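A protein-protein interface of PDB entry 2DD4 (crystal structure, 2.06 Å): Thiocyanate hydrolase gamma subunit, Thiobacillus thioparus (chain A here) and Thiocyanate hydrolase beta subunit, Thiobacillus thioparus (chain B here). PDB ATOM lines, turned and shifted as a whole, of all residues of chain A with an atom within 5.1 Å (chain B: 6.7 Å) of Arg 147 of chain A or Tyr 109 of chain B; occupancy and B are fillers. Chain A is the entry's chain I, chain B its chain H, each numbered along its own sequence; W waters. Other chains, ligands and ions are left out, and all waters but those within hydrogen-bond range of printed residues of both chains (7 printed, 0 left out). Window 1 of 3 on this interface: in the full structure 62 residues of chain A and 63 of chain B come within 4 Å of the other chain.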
ATOM      1  N   CYS A 131       9.058 -33.303   1.710  1.00  0.00           N
ATOM      2  CA  CYS A 131       8.699 -31.941   2.087  1.00  0.00           C
ATOM      3  C   CYS A 131       7.185 -31.787   2.157  1.00  0.00           C
ATOM      4  O   CYS A 131       6.529 -32.489   2.924  1.00  0.00           O
ATOM      5  CB  CYS A 131       9.318 -30.921   1.115  1.00  0.00           C
ATOM      6  SG  CYS A 131       9.423 -31.421  -0.625  1.00  0.00           S
ATOM      7  N   SER A 132       6.617 -30.878   1.376  1.00  0.00           N
ATOM      8  CA  SER A 132       5.170 -30.714   1.419  1.00  0.00           C
ATOM      9  C   SER A 132       4.547 -30.417   0.061  1.00  0.00           C
ATOM     10  O   SER A 132       3.573 -29.670  -0.029  1.00  0.00           O
ATOM     11  CB  SER A 132       4.800 -29.618   2.418  1.00  0.00           C
ATOM     12  OG  SER A 132       5.458 -28.410   2.100  1.00  0.00           O
ATOM     13  N   GLN A 141      -3.520 -23.841  -0.370  1.00  0.00           N
ATOM     14  CA  GLN A 141      -2.349 -24.050   0.479  1.00  0.00           C
ATOM     15  C   GLN A 141      -2.464 -25.338   1.294  1.00  0.00           C
ATOM     16  O   GLN A 141      -3.561 -25.756   1.669  1.00  0.00           O
ATOM     17  CB  GLN A 141      -2.166 -22.839   1.404  1.00  0.00           C
ATOM     18  CG  GLN A 141      -0.825 -22.776   2.121  1.00  0.00           C
ATOM     19  CD  GLN A 141       0.372 -22.811   1.174  1.00  0.00           C
ATOM     20  OE1 GLN A 141       0.850 -23.886   0.792  1.00  0.00           O
ATOM     21  NE2 GLN A 141       0.856 -21.632   0.789  1.00  0.00           N
ATOM     22  N   SER A 142      -1.324 -25.963   1.571  1.00  0.00           N
ATOM     23  CA  SER A 142      -1.295 -27.218   2.323  1.00  0.00           C
ATOM     24  C   SER A 142      -1.605 -27.065   3.810  1.00  0.00           C
ATOM     25  O   SER A 142      -1.315 -26.032   4.411  1.00  0.00           O
ATOM     26  CB  SER A 142       0.077 -27.880   2.173  1.00  0.00           C
ATOM     27  OG  SER A 142       1.094 -27.064   2.735  1.00  0.00           O
ATOM     28  N   PRO A 143      -2.201 -28.105   4.421  1.00  0.00           N
ATOM     29  CA  PRO A 143      -2.551 -28.104   5.847  1.00  0.00           C
ATOM     30  C   PRO A 143      -1.267 -28.152   6.675  1.00  0.00           C
ATOM     31  O   PRO A 143      -0.260 -28.689   6.223  1.00  0.00           O
ATOM     32  CB  PRO A 143      -3.360 -29.390   6.011  1.00  0.00           C
ATOM     33  CG  PRO A 143      -3.907 -29.643   4.633  1.00  0.00           C
ATOM     34  CD  PRO A 143      -2.744 -29.301   3.755  1.00  0.00           C
ATOM     35  N   GLU A 144      -1.308 -27.604   7.885  1.00  0.00           N
ATOM     36  CA  GLU A 144      -0.131 -27.607   8.750  1.00  0.00           C
ATOM     37  C   GLU A 144       0.358 -29.034   9.007  1.00  0.00           C
ATOM     38  O   GLU A 144       1.553 -29.316   8.895  1.00  0.00           O
ATOM     39  CB  GLU A 144      -0.457 -26.919  10.083  1.00  0.00           C
ATOM     40  CG  GLU A 144       0.719 -26.816  11.064  1.00  0.00           C
ATOM     41  CD  GLU A 144       1.761 -25.785  10.643  1.00  0.00           C
ATOM     42  OE1 GLU A 144       1.548 -25.077   9.634  1.00  0.00           O
ATOM     43  OE2 GLU A 144       2.796 -25.680  11.331  1.00  0.00           O
ATOM     44  N   TRP A 145      -0.562 -29.938   9.338  1.00  0.00           N
ATOM     45  CA  TRP A 145      -0.189 -31.324   9.624  1.00  0.00           C
ATOM     46  C   TRP A 145       0.411 -32.071   8.431  1.00  0.00           C
ATOM     47  O   TRP A 145       1.221 -32.985   8.607  1.00  0.00           O
ATOM     48  CB  TRP A 145      -1.390 -32.106  10.173  1.00  0.00           C
ATOM     49  CG  TRP A 145      -2.652 -31.981   9.363  1.00  0.00           C
ATOM     50  CD1 TRP A 145      -3.666 -31.091   9.560  1.00  0.00           C
ATOM     51  CD2 TRP A 145      -3.024 -32.770   8.224  1.00  0.00           C
ATOM     52  NE1 TRP A 145      -4.650 -31.274   8.613  1.00  0.00           N
ATOM     53  CE2 TRP A 145      -4.279 -32.299   7.781  1.00  0.00           C
ATOM     54  CE3 TRP A 145      -2.417 -33.831   7.535  1.00  0.00           C
ATOM     55  CZ2 TRP A 145      -4.944 -32.850   6.676  1.00  0.00           C
ATOM     56  CZ3 TRP A 145      -3.078 -34.381   6.434  1.00  0.00           C
ATOM     57  CH2 TRP A 145      -4.329 -33.887   6.018  1.00  0.00           C
ATOM     58  N   TYR A 146       0.014 -31.679   7.224  1.00  0.00           N
ATOM     59  CA  TYR A 146       0.509 -32.300   5.995  1.00  0.00           C
ATOM     60  C   TYR A 146       2.009 -32.042   5.845  1.00  0.00           C
ATOM     61  O   TYR A 146       2.735 -32.838   5.248  1.00  0.00           O
ATOM     62  CB  TYR A 146      -0.231 -31.711   4.790  1.00  0.00           C
ATOM     63  CG  TYR A 146       0.158 -32.294   3.447  1.00  0.00           C
ATOM     64  CD1 TYR A 146      -0.412 -33.481   2.988  1.00  0.00           C
ATOM     65  CD2 TYR A 146       1.072 -31.640   2.621  1.00  0.00           C
ATOM     66  CE1 TYR A 146      -0.090 -34.001   1.736  1.00  0.00           C
ATOM     67  CE2 TYR A 146       1.407 -32.152   1.367  1.00  0.00           C
ATOM     68  CZ  TYR A 146       0.820 -33.332   0.931  1.00  0.00           C
ATOM     69  OH  TYR A 146       1.139 -33.844  -0.307  1.00  0.00           O
ATOM     70  N   ARG A 147       2.458 -30.916   6.392  1.00  0.00           N
ATOM     71  CA  ARG A 147       3.863 -30.515   6.329  1.00  0.00           C
ATOM     72  C   ARG A 147       4.678 -31.128   7.460  1.00  0.00           C
ATOM     73  O   ARG A 147       5.908 -31.095   7.430  1.00  0.00           O
ATOM     74  CB  ARG A 147       3.981 -28.990   6.450  1.00  0.00           C
ATOM     75  CG  ARG A 147       3.052 -28.192   5.555  1.00  0.00           C
ATOM     76  CD  ARG A 147       3.029 -26.718   5.968  1.00  0.00           C
ATOM     77  NE  ARG A 147       2.096 -25.948   5.153  1.00  0.00           N
ATOM     78  CZ  ARG A 147       1.811 -24.660   5.336  1.00  0.00           C
ATOM     79  NH1 ARG A 147       2.390 -23.972   6.312  1.00  0.00           N
ATOM     80  NH2 ARG A 147       0.936 -24.064   4.539  1.00  0.00           N
ATOM     81  N   SER A 148       4.001 -31.685   8.459  1.00  0.00           N
ATOM     82  CA  SER A 148       4.704 -32.233   9.616  1.00  0.00           C
ATOM     83  C   SER A 148       5.585 -33.446   9.360  1.00  0.00           C
ATOM     84  O   SER A 148       5.260 -34.318   8.551  1.00  0.00           O
ATOM     85  CB  SER A 148       3.711 -32.578  10.735  1.00  0.00           C
ATOM     86  OG  SER A 148       3.030 -33.794  10.465  1.00  0.00           O
ATOM     87  N   PRO A 149       6.738 -33.500  10.044  1.00  0.00           N
ATOM     88  CA  PRO A 149       7.672 -34.619   9.906  1.00  0.00           C
ATOM     89  C   PRO A 149       6.933 -35.907  10.287  1.00  0.00           C
ATOM     90  O   PRO A 149       7.171 -36.971   9.721  1.00  0.00           O
ATOM     91  CB  PRO A 149       8.766 -34.275  10.915  1.00  0.00           C
ATOM     92  CG  PRO A 149       8.802 -32.777  10.863  1.00  0.00           C
ATOM     93  CD  PRO A 149       7.334 -32.406  10.838  1.00  0.00           C
ATOM     94  N   ARG A 152       4.759 -37.127   7.508  1.00  0.00           N
ATOM     95  CA  ARG A 152       5.705 -37.519   6.463  1.00  0.00           C
ATOM     96  C   ARG A 152       6.491 -38.791   6.772  1.00  0.00           C
ATOM     97  O   ARG A 152       6.909 -39.504   5.864  1.00  0.00           O
ATOM     98  CB  ARG A 152       6.668 -36.356   6.173  1.00  0.00           C
ATOM     99  CG  ARG A 152       5.986 -35.140   5.520  1.00  0.00           C
ATOM    100  CD  ARG A 152       6.889 -33.914   5.569  1.00  0.00           C
ATOM    101  NE  ARG A 152       8.237 -34.256   5.142  1.00  0.00           N
ATOM    102  CZ  ARG A 152       9.344 -33.704   5.628  1.00  0.00           C
ATOM    103  NH1 ARG A 152       9.269 -32.766   6.566  1.00  0.00           N
ATOM    104  NH2 ARG A 152      10.528 -34.114   5.191  1.00  0.00           N
ATOM    105  N   LYS B  63      -2.969 -24.726  11.480  1.00  0.00           N
ATOM    106  CA  LYS B  63      -2.290 -23.558  12.036  1.00  0.00           C
ATOM    107  C   LYS B  63      -2.571 -22.350  11.157  1.00  0.00           C
ATOM    108  O   LYS B  63      -2.443 -22.425   9.932  1.00  0.00           O
ATOM    109  CB  LYS B  63      -0.770 -23.753  12.126  1.00  0.00           C
ATOM    110  CG  LYS B  63      -0.081 -22.609  12.901  1.00  0.00           C
ATOM    111  CD  LYS B  63       1.445 -22.707  12.907  1.00  0.00           C
ATOM    112  CE  LYS B  63       2.055 -22.181  11.604  1.00  0.00           C
ATOM    113  NZ  LYS B  63       1.804 -20.724  11.412  1.00  0.00           N
ATOM    114  N   GLU B  65      -2.072 -18.967   9.188  1.00  0.00           N
ATOM    115  CA  GLU B  65      -0.915 -18.489   8.449  1.00  0.00           C
ATOM    116  C   GLU B  65      -0.475 -17.127   8.992  1.00  0.00           C
ATOM    117  O   GLU B  65      -1.287 -16.206   9.108  1.00  0.00           O
ATOM    118  CB  GLU B  65      -1.260 -18.371   6.959  1.00  0.00           C
ATOM    119  CG  GLU B  65      -0.152 -17.756   6.104  1.00  0.00           C
ATOM    120  CD  GLU B  65      -0.553 -17.616   4.642  1.00  0.00           C
ATOM    121  OE1 GLU B  65      -1.678 -17.137   4.376  1.00  0.00           O
ATOM    122  OE2 GLU B  65       0.257 -17.974   3.761  1.00  0.00           O
ATOM    123  N   GLU B  66       0.802 -17.010   9.352  1.00  0.00           N
ATOM    124  CA  GLU B  66       1.339 -15.746   9.846  1.00  0.00           C
ATOM    125  C   GLU B  66       1.498 -14.835   8.634  1.00  0.00           C
ATOM    126  O   GLU B  66       1.736 -15.311   7.523  1.00  0.00           O
ATOM    127  CB  GLU B  66       2.722 -15.946  10.479  1.00  0.00           C
ATOM    128  CG  GLU B  66       2.758 -16.806  11.732  1.00  0.00           C
ATOM    129  CD  GLU B  66       2.566 -16.009  13.010  1.00  0.00           C
ATOM    130  OE1 GLU B  66       2.352 -14.781  12.927  1.00  0.00           O
ATOM    131  OE2 GLU B  66       2.631 -16.615  14.104  1.00  0.00           O
ATOM    132  N   TRP B  68       3.947 -12.945   8.025  1.00  0.00           N
ATOM    133  CA  TRP B  68       5.316 -13.086   7.531  1.00  0.00           C
ATOM    134  C   TRP B  68       5.536 -14.373   6.744  1.00  0.00           C
ATOM    135  O   TRP B  68       6.434 -14.440   5.903  1.00  0.00           O
ATOM    136  CB  TRP B  68       6.343 -12.977   8.674  1.00  0.00           C
ATOM    137  CG  TRP B  68       6.438 -14.158   9.603  1.00  0.00           C
ATOM    138  CD1 TRP B  68       5.808 -14.312  10.808  1.00  0.00           C
ATOM    139  CD2 TRP B  68       7.256 -15.324   9.425  1.00  0.00           C
ATOM    140  NE1 TRP B  68       6.190 -15.498  11.396  1.00  0.00           N
ATOM    141  CE2 TRP B  68       7.074 -16.139  10.567  1.00  0.00           C
ATOM    142  CE3 TRP B  68       8.125 -15.756   8.412  1.00  0.00           C
ATOM    143  CZ2 TRP B  68       7.733 -17.367  10.726  1.00  0.00           C
ATOM    144  CZ3 TRP B  68       8.785 -16.985   8.570  1.00  0.00           C
ATOM    145  CH2 TRP B  68       8.580 -17.771   9.721  1.00  0.00           C
ATOM    146  N   GLU B  69       4.719 -15.390   7.006  1.00  0.00           N
ATOM    147  CA  GLU B  69       4.830 -16.653   6.280  1.00  0.00           C
ATOM    148  C   GLU B  69       4.287 -16.457   4.862  1.00  0.00           C
ATOM    149  O   GLU B  69       4.877 -16.930   3.884  1.00  0.00           O
ATOM    150  CB  GLU B  69       4.052 -17.767   6.999  1.00  0.00           C
ATOM    151  CG  GLU B  69       4.606 -18.111   8.387  1.00  0.00           C
ATOM    152  CD  GLU B  69       3.832 -19.219   9.082  1.00  0.00           C
ATOM    153  OE1 GLU B  69       2.587 -19.194   9.032  1.00  0.00           O
ATOM    154  OE2 GLU B  69       4.468 -20.105   9.697  1.00  0.00           O
ATOM    155  N   LEU B  70       3.167 -15.752   4.746  1.00  0.00           N
ATOM    156  CA  LEU B  70       2.590 -15.499   3.427  1.00  0.00           C
ATOM    157  C   LEU B  70       3.572 -14.684   2.590  1.00  0.00           C
ATOM    158  O   LEU B  70       3.770 -14.966   1.407  1.00  0.00           O
ATOM    159  CB  LEU B  70       1.264 -14.739   3.541  1.00  0.00           C
ATOM    160  CG  LEU B  70       0.687 -14.220   2.215  1.00  0.00           C
ATOM    161  CD1 LEU B  70       0.475 -15.383   1.241  1.00  0.00           C
ATOM    162  CD2 LEU B  70      -0.626 -13.492   2.477  1.00  0.00           C
ATOM    163  N   THR B  72       6.801 -14.562   2.981  1.00  0.00           N
ATOM    164  CA  THR B  72       7.960 -15.403   2.705  1.00  0.00           C
ATOM    165  C   THR B  72       7.655 -16.306   1.505  1.00  0.00           C
ATOM    166  O   THR B  72       8.467 -16.441   0.589  1.00  0.00           O
ATOM    167  CB  THR B  72       8.318 -16.282   3.926  1.00  0.00           C
ATOM    168  OG1 THR B  72       8.823 -15.450   4.976  1.00  0.00           O
ATOM    169  CG2 THR B  72       9.375 -17.320   3.557  1.00  0.00           C
ATOM    170  N   PHE B  73       6.477 -16.919   1.518  1.00  0.00           N
ATOM    171  CA  PHE B  73       6.072 -17.796   0.422  1.00  0.00           C
ATOM    172  C   PHE B  73       6.133 -17.025  -0.901  1.00  0.00           C
ATOM    173  O   PHE B  73       6.723 -17.495  -1.874  1.00  0.00           O
ATOM    174  CB  PHE B  73       4.653 -18.322   0.661  1.00  0.00           C
ATOM    175  CG  PHE B  73       4.160 -19.239  -0.421  1.00  0.00           C
ATOM    176  CD1 PHE B  73       4.795 -20.454  -0.665  1.00  0.00           C
ATOM    177  CD2 PHE B  73       3.077 -18.879  -1.217  1.00  0.00           C
ATOM    178  CE1 PHE B  73       4.360 -21.299  -1.688  1.00  0.00           C
ATOM    179  CE2 PHE B  73       2.632 -19.718  -2.249  1.00  0.00           C
ATOM    180  CZ  PHE B  73       3.277 -20.929  -2.481  1.00  0.00           C
ATOM    181  N   ALA B  74       5.529 -15.838  -0.925  1.00  0.00           N
ATOM    182  CA  ALA B  74       5.517 -15.006  -2.125  1.00  0.00           C
ATOM    183  C   ALA B  74       6.935 -14.640  -2.567  1.00  0.00           C
ATOM    184  O   ALA B  74       7.241 -14.643  -3.760  1.00  0.00           O
ATOM    185  CB  ALA B  74       4.701 -13.738  -1.873  1.00  0.00           C
ATOM    186  N   CYS B  76       9.722 -16.317  -2.030  1.00  0.00           N
ATOM    187  CA  CYS B  76      10.388 -17.482  -2.581  1.00  0.00           C
ATOM    188  C   CYS B  76       9.917 -17.816  -3.993  1.00  0.00           C
ATOM    189  O   CYS B  76      10.729 -18.158  -4.849  1.00  0.00           O
ATOM    190  CB  CYS B  76      10.214 -18.675  -1.642  1.00  0.00           C
ATOM    191  SG  CYS B  76      11.179 -18.495  -0.112  1.00  0.00           S
ATOM    192  N   TYR B 103      16.953 -28.280  10.599  1.00  0.00           N
ATOM    193  CA  TYR B 103      15.861 -28.914   9.859  1.00  0.00           C
ATOM    194  C   TYR B 103      14.663 -29.295  10.734  1.00  0.00           C
ATOM    195  O   TYR B 103      13.513 -29.126  10.327  1.00  0.00           O
ATOM    196  CB  TYR B 103      16.351 -30.166   9.126  1.00  0.00           C
ATOM    197  CG  TYR B 103      15.281 -30.760   8.234  1.00  0.00           C
ATOM    198  CD1 TYR B 103      14.768 -30.033   7.159  1.00  0.00           C
ATOM    199  CD2 TYR B 103      14.754 -32.025   8.484  1.00  0.00           C
ATOM    200  CE1 TYR B 103      13.755 -30.548   6.357  1.00  0.00           C
ATOM    201  CE2 TYR B 103      13.738 -32.551   7.685  1.00  0.00           C
ATOM    202  CZ  TYR B 103      13.245 -31.806   6.627  1.00  0.00           C
ATOM    203  OH  TYR B 103      12.236 -32.308   5.842  1.00  0.00           O
ATOM    204  N   MET B 106      13.877 -25.777  13.896  1.00  0.00           N
ATOM    205  CA  MET B 106      13.239 -24.523  13.508  1.00  0.00           C
ATOM    206  C   MET B 106      11.923 -24.754  12.772  1.00  0.00           C
ATOM    207  O   MET B 106      11.638 -25.864  12.321  1.00  0.00           O
ATOM    208  CB  MET B 106      14.192 -23.712  12.631  1.00  0.00           C
ATOM    209  CG  MET B 106      15.332 -23.061  13.399  1.00  0.00           C
ATOM    210  SD  MET B 106      14.801 -21.574  14.306  1.00  0.00           S
ATOM    211  CE  MET B 106      15.005 -20.333  13.028  1.00  0.00           C
ATOM    212  N   PRO B 107      11.100 -23.699  12.645  1.00  0.00           N
ATOM    213  CA  PRO B 107       9.812 -23.811  11.958  1.00  0.00           C
ATOM    214  C   PRO B 107       9.946 -23.957  10.447  1.00  0.00           C
ATOM    215  O   PRO B 107      10.908 -23.481   9.847  1.00  0.00           O
ATOM    216  CB  PRO B 107       9.098 -22.507  12.325  1.00  0.00           C
ATOM    217  CG  PRO B 107       9.791 -22.049  13.581  1.00  0.00           C
ATOM    218  CD  PRO B 107      11.227 -22.384  13.297  1.00  0.00           C
ATOM    219  N   TYR B 108       8.955 -24.620   9.857  1.00  0.00           N
ATOM    220  CA  TYR B 108       8.850 -24.842   8.417  1.00  0.00           C
ATOM    221  C   TYR B 108       9.177 -23.566   7.633  1.00  0.00           C
ATOM    222  O   TYR B 108      10.145 -23.523   6.872  1.00  0.00           O
ATOM    223  CB  TYR B 108       7.418 -25.297   8.122  1.00  0.00           C
ATOM    224  CG  TYR B 108       6.994 -25.399   6.673  1.00  0.00           C
ATOM    225  CD1 TYR B 108       7.296 -26.532   5.907  1.00  0.00           C
ATOM    226  CD2 TYR B 108       6.174 -24.423   6.106  1.00  0.00           C
ATOM    227  CE1 TYR B 108       6.769 -26.696   4.620  1.00  0.00           C
ATOM    228  CE2 TYR B 108       5.645 -24.577   4.823  1.00  0.00           C
ATOM    229  CZ  TYR B 108       5.941 -25.716   4.091  1.00  0.00           C
ATOM    230  OH  TYR B 108       5.364 -25.887   2.850  1.00  0.00           O
ATOM    231  N   TYR B 109       8.370 -22.525   7.816  1.00  0.00           N
ATOM    232  CA  TYR B 109       8.612 -21.277   7.107  1.00  0.00           C
ATOM    233  C   TYR B 109       9.859 -20.533   7.570  1.00  0.00           C
ATOM    234  O   TYR B 109      10.366 -19.660   6.862  1.00  0.00           O
ATOM    235  CB  TYR B 109       7.382 -20.372   7.178  1.00  0.00           C
ATOM    236  CG  TYR B 109       6.454 -20.594   6.008  1.00  0.00           C
ATOM    237  CD1 TYR B 109       6.919 -20.449   4.700  1.00  0.00           C
ATOM    238  CD2 TYR B 109       5.121 -20.959   6.198  1.00  0.00           C
ATOM    239  CE1 TYR B 109       6.082 -20.662   3.608  1.00  0.00           C
ATOM    240  CE2 TYR B 109       4.272 -21.176   5.107  1.00  0.00           C
ATOM    241  CZ  TYR B 109       4.763 -21.025   3.818  1.00  0.00           C
ATOM    242  OH  TYR B 109       3.945 -21.235   2.734  1.00  0.00           O
ATOM    243  N   GLY B 110      10.358 -20.880   8.752  1.00  0.00           N
ATOM    244  CA  GLY B 110      11.576 -20.248   9.227  1.00  0.00           C
ATOM    245  C   GLY B 110      12.705 -20.674   8.296  1.00  0.00           C
ATOM    246  O   GLY B 110      13.580 -19.881   7.953  1.00  0.00           O
ATOM    247  N   ARG B 111      12.678 -21.936   7.873  1.00  0.00           N
ATOM    248  CA  ARG B 111      13.698 -22.468   6.971  1.00  0.00           C
ATOM    249  C   ARG B 111      13.556 -21.868   5.570  1.00  0.00           C
ATOM    250  O   ARG B 111      14.549 -21.645   4.883  1.00  0.00           O
ATOM    251  CB  ARG B 111      13.604 -23.998   6.918  1.00  0.00           C
ATOM    252  CG  ARG B 111      13.896 -24.658   8.273  1.00  0.00           C
ATOM    253  CD  ARG B 111      13.940 -26.183   8.203  1.00  0.00           C
ATOM    254  NE  ARG B 111      12.659 -26.773   7.820  1.00  0.00           N
ATOM    255  CZ  ARG B 111      12.336 -27.127   6.578  1.00  0.00           C
ATOM    256  NH1 ARG B 111      13.198 -26.955   5.583  1.00  0.00           N
ATOM    257  NH2 ARG B 111      11.152 -27.673   6.333  1.00  0.00           N
ATOM    258  N   TRP B 112      12.324 -21.609   5.148  1.00  0.00           N
ATOM    259  CA  TRP B 112      12.090 -20.990   3.839  1.00  0.00           C
ATOM    260  C   TRP B 112      12.741 -19.608   3.828  1.00  0.00           C
ATOM    261  O   TRP B 112      13.480 -19.252   2.909  1.00  0.00           O
ATOM    262  CB  TRP B 112      10.599 -20.771   3.587  1.00  0.00           C
ATOM    263  CG  TRP B 112       9.798 -21.944   3.150  1.00  0.00           C
ATOM    264  CD1 TRP B 112       9.538 -23.078   3.861  1.00  0.00           C
ATOM    265  CD2 TRP B 112       9.037 -22.043   1.941  1.00  0.00           C
ATOM    266  NE1 TRP B 112       8.651 -23.874   3.174  1.00  0.00           N
ATOM    267  CE2 TRP B 112       8.327 -23.261   1.992  1.00  0.00           C
ATOM    268  CE3 TRP B 112       8.883 -21.216   0.818  1.00  0.00           C
ATOM    269  CZ2 TRP B 112       7.470 -23.673   0.965  1.00  0.00           C
ATOM    270  CZ3 TRP B 112       8.032 -21.624  -0.205  1.00  0.00           C
ATOM    271  CH2 TRP B 112       7.335 -22.844  -0.122  1.00  0.00           C
ATOM    272  N   LEU B 113      12.431 -18.829   4.859  1.00  0.00           N
ATOM    273  CA  LEU B 113      12.932 -17.464   4.992  1.00  0.00           C
ATOM    274  C   LEU B 113      14.449 -17.367   5.075  1.00  0.00           C
ATOM    275  O   LEU B 113      15.062 -16.554   4.381  1.00  0.00           O
ATOM    276  CB  LEU B 113      12.294 -16.796   6.215  1.00  0.00           C
ATOM    277  CG  LEU B 113      12.673 -15.335   6.482  1.00  0.00           C
ATOM    278  CD1 LEU B 113      12.491 -14.500   5.216  1.00  0.00           C
ATOM    279  CD2 LEU B 113      11.807 -14.797   7.615  1.00  0.00           C
ATOM    280  N   LEU B 114      15.054 -18.180   5.935  1.00  0.00           N
ATOM    281  CA  LEU B 114      16.506 -18.180   6.079  1.00  0.00           C
ATOM    282  C   LEU B 114      17.158 -18.531   4.744  1.00  0.00           C
ATOM    283  O   LEU B 114      18.180 -17.964   4.362  1.00  0.00           O
ATOM    284  CB  LEU B 114      16.936 -19.213   7.123  1.00  0.00           C
ATOM    285  CG  LEU B 114      16.625 -18.942   8.595  1.00  0.00           C
ATOM    286  CD1 LEU B 114      16.834 -20.224   9.401  1.00  0.00           C
ATOM    287  CD2 LEU B 114      17.523 -17.828   9.110  1.00  0.00           C
HETATM  288  O   HOH W   1       3.612 -23.913   1.772  1.00  0.00           O
HETATM  289  O   HOH W   2      -0.090 -23.391   8.492  1.00  0.00           O
HETATM  290  O   HOH W   3       1.412 -21.363   7.462  1.00  0.00           O
HETATM  291  O   HOH W   4      -3.353 -25.766   8.637  1.00  0.00           O
HETATM  292  O   HOH W   5      10.831 -31.094   8.581  1.00  0.00           O
HETATM  293  O   HOH W   6       1.627 -20.137   3.188  1.00  0.00           O
HETATM  294  O   HOH W   7       0.291 -18.779   1.062  1.00  0.00           O
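NE2 of Gln 141 of chain A touches OH of Tyr 109 of chain B, at 3.7 Å. CE of Lys 63 of chain B touches OE1 of Glu 144 of chain A, 3.5 Å away. CD of Arg 147 of chain A touches CE2 of Tyr 108 of chain B, 3.6 Å away. Arg 147 of chain A touches Tyr 109 of chain B (NH1 to CE2, 3.6 Å).
The side-chain hydroxyl of Tyr 103 of chain B is in hydrogen-bond range of the guanidinium group of Arg 152 of chain A (2.6 Å). OH of Tyr 108 of chain B lies within hydrogen-bond range of OG of Ser 132 of chain A.
Of the 20 printed residues of chain B, 4 touch a printed residue of chain A. Printed residues of chain B that touch a printed residue of chain A: Lys 63, Tyr 103, Tyr 108 and Tyr 109. Hydrophobic or aromatic side chains of chain B that line the printed part of chain A: Tyr 103, Tyr 108 and Tyr 109. Of the 12 printed residues of chain A, 5 touch a printed residue of chain B. Along chain A the printed residues that touch a printed residue of chain B span positions 132 to 152.
Water W2 lies within hydrogen-bond range of the side-chain carboxylate (OE1) of Glu 144 of chain A (2.6 Å), the backbone carbonyl oxygen (O) of Lys 63 of chain B (2.9 Å) and the guanidinium group (NH1) of Arg 147 of chain A (3.4 Å). Water W7 lies within hydrogen-bond range of the side-chain carboxylate (OE2) of Glu 65 of chain B (2.8 Å) and the side-chain amide nitrogen (NE2) of Gln 141 of chain A (2.9 Å). Water W4 bridges N of Glu 144 of chain A (2.9 Å) and N of Lys 63 of chain B (3.1 Å). Water W1 lies within hydrogen-bond range of the side-chain hydroxyl of Tyr 108 of chain B (2.9 Å), the side-chain hydroxyl of Tyr 109 of chain B (2.9 Å) and the side-chain amide oxygen of Gln 141 of chain A (2.9 Å). Water W3 bridges the side-chain carboxylate (OE1) of Glu 69 of chain B and the guanidinium group (NH1) of Arg 147 of chain A. Water W5 lies within hydrogen-bond range of the guanidinium group (NH1) of Arg 152 of chain A and the side-chain hydroxyl (OH) of Tyr 103 of chain B.
Arg 147 of chain A touches just these residues of chain B: Tyr 108 (3.6 Å) and Tyr 109 (3.6 Å). Tyr 109 of chain B touches just these residues of chain A: Gln 141 and Arg 147. Printed residues of chain B within 4 Å of Ser 132 of chain A: Tyr 108 (2.6 Å). Of the printed residues of chain B, Arg 152 of chain A touches Tyr 103. The nearest printed residue of chain A that does not touch Tyr 109 of chain B is Glu 144 of chain A (6.4 Å).
The side-chain carboxylate of Glu 69 of chain B lies within salt-bridge range of the side-chain amino group of Lys 63 of chain B, 2.9 Å away. The backbone carbonyl oxygen of Cys 131 of chain A sits close to the guanidinium group of Arg 152 of chain A (3.3 Å). The side-chain hydroxyl of Ser 142 of chain A is in hydrogen-bond range of the guanidinium group of Arg 147 of chain A. OE1 of Glu 144 of chain A lies within salt-bridge range of NH1 of Arg 147 of chain A.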
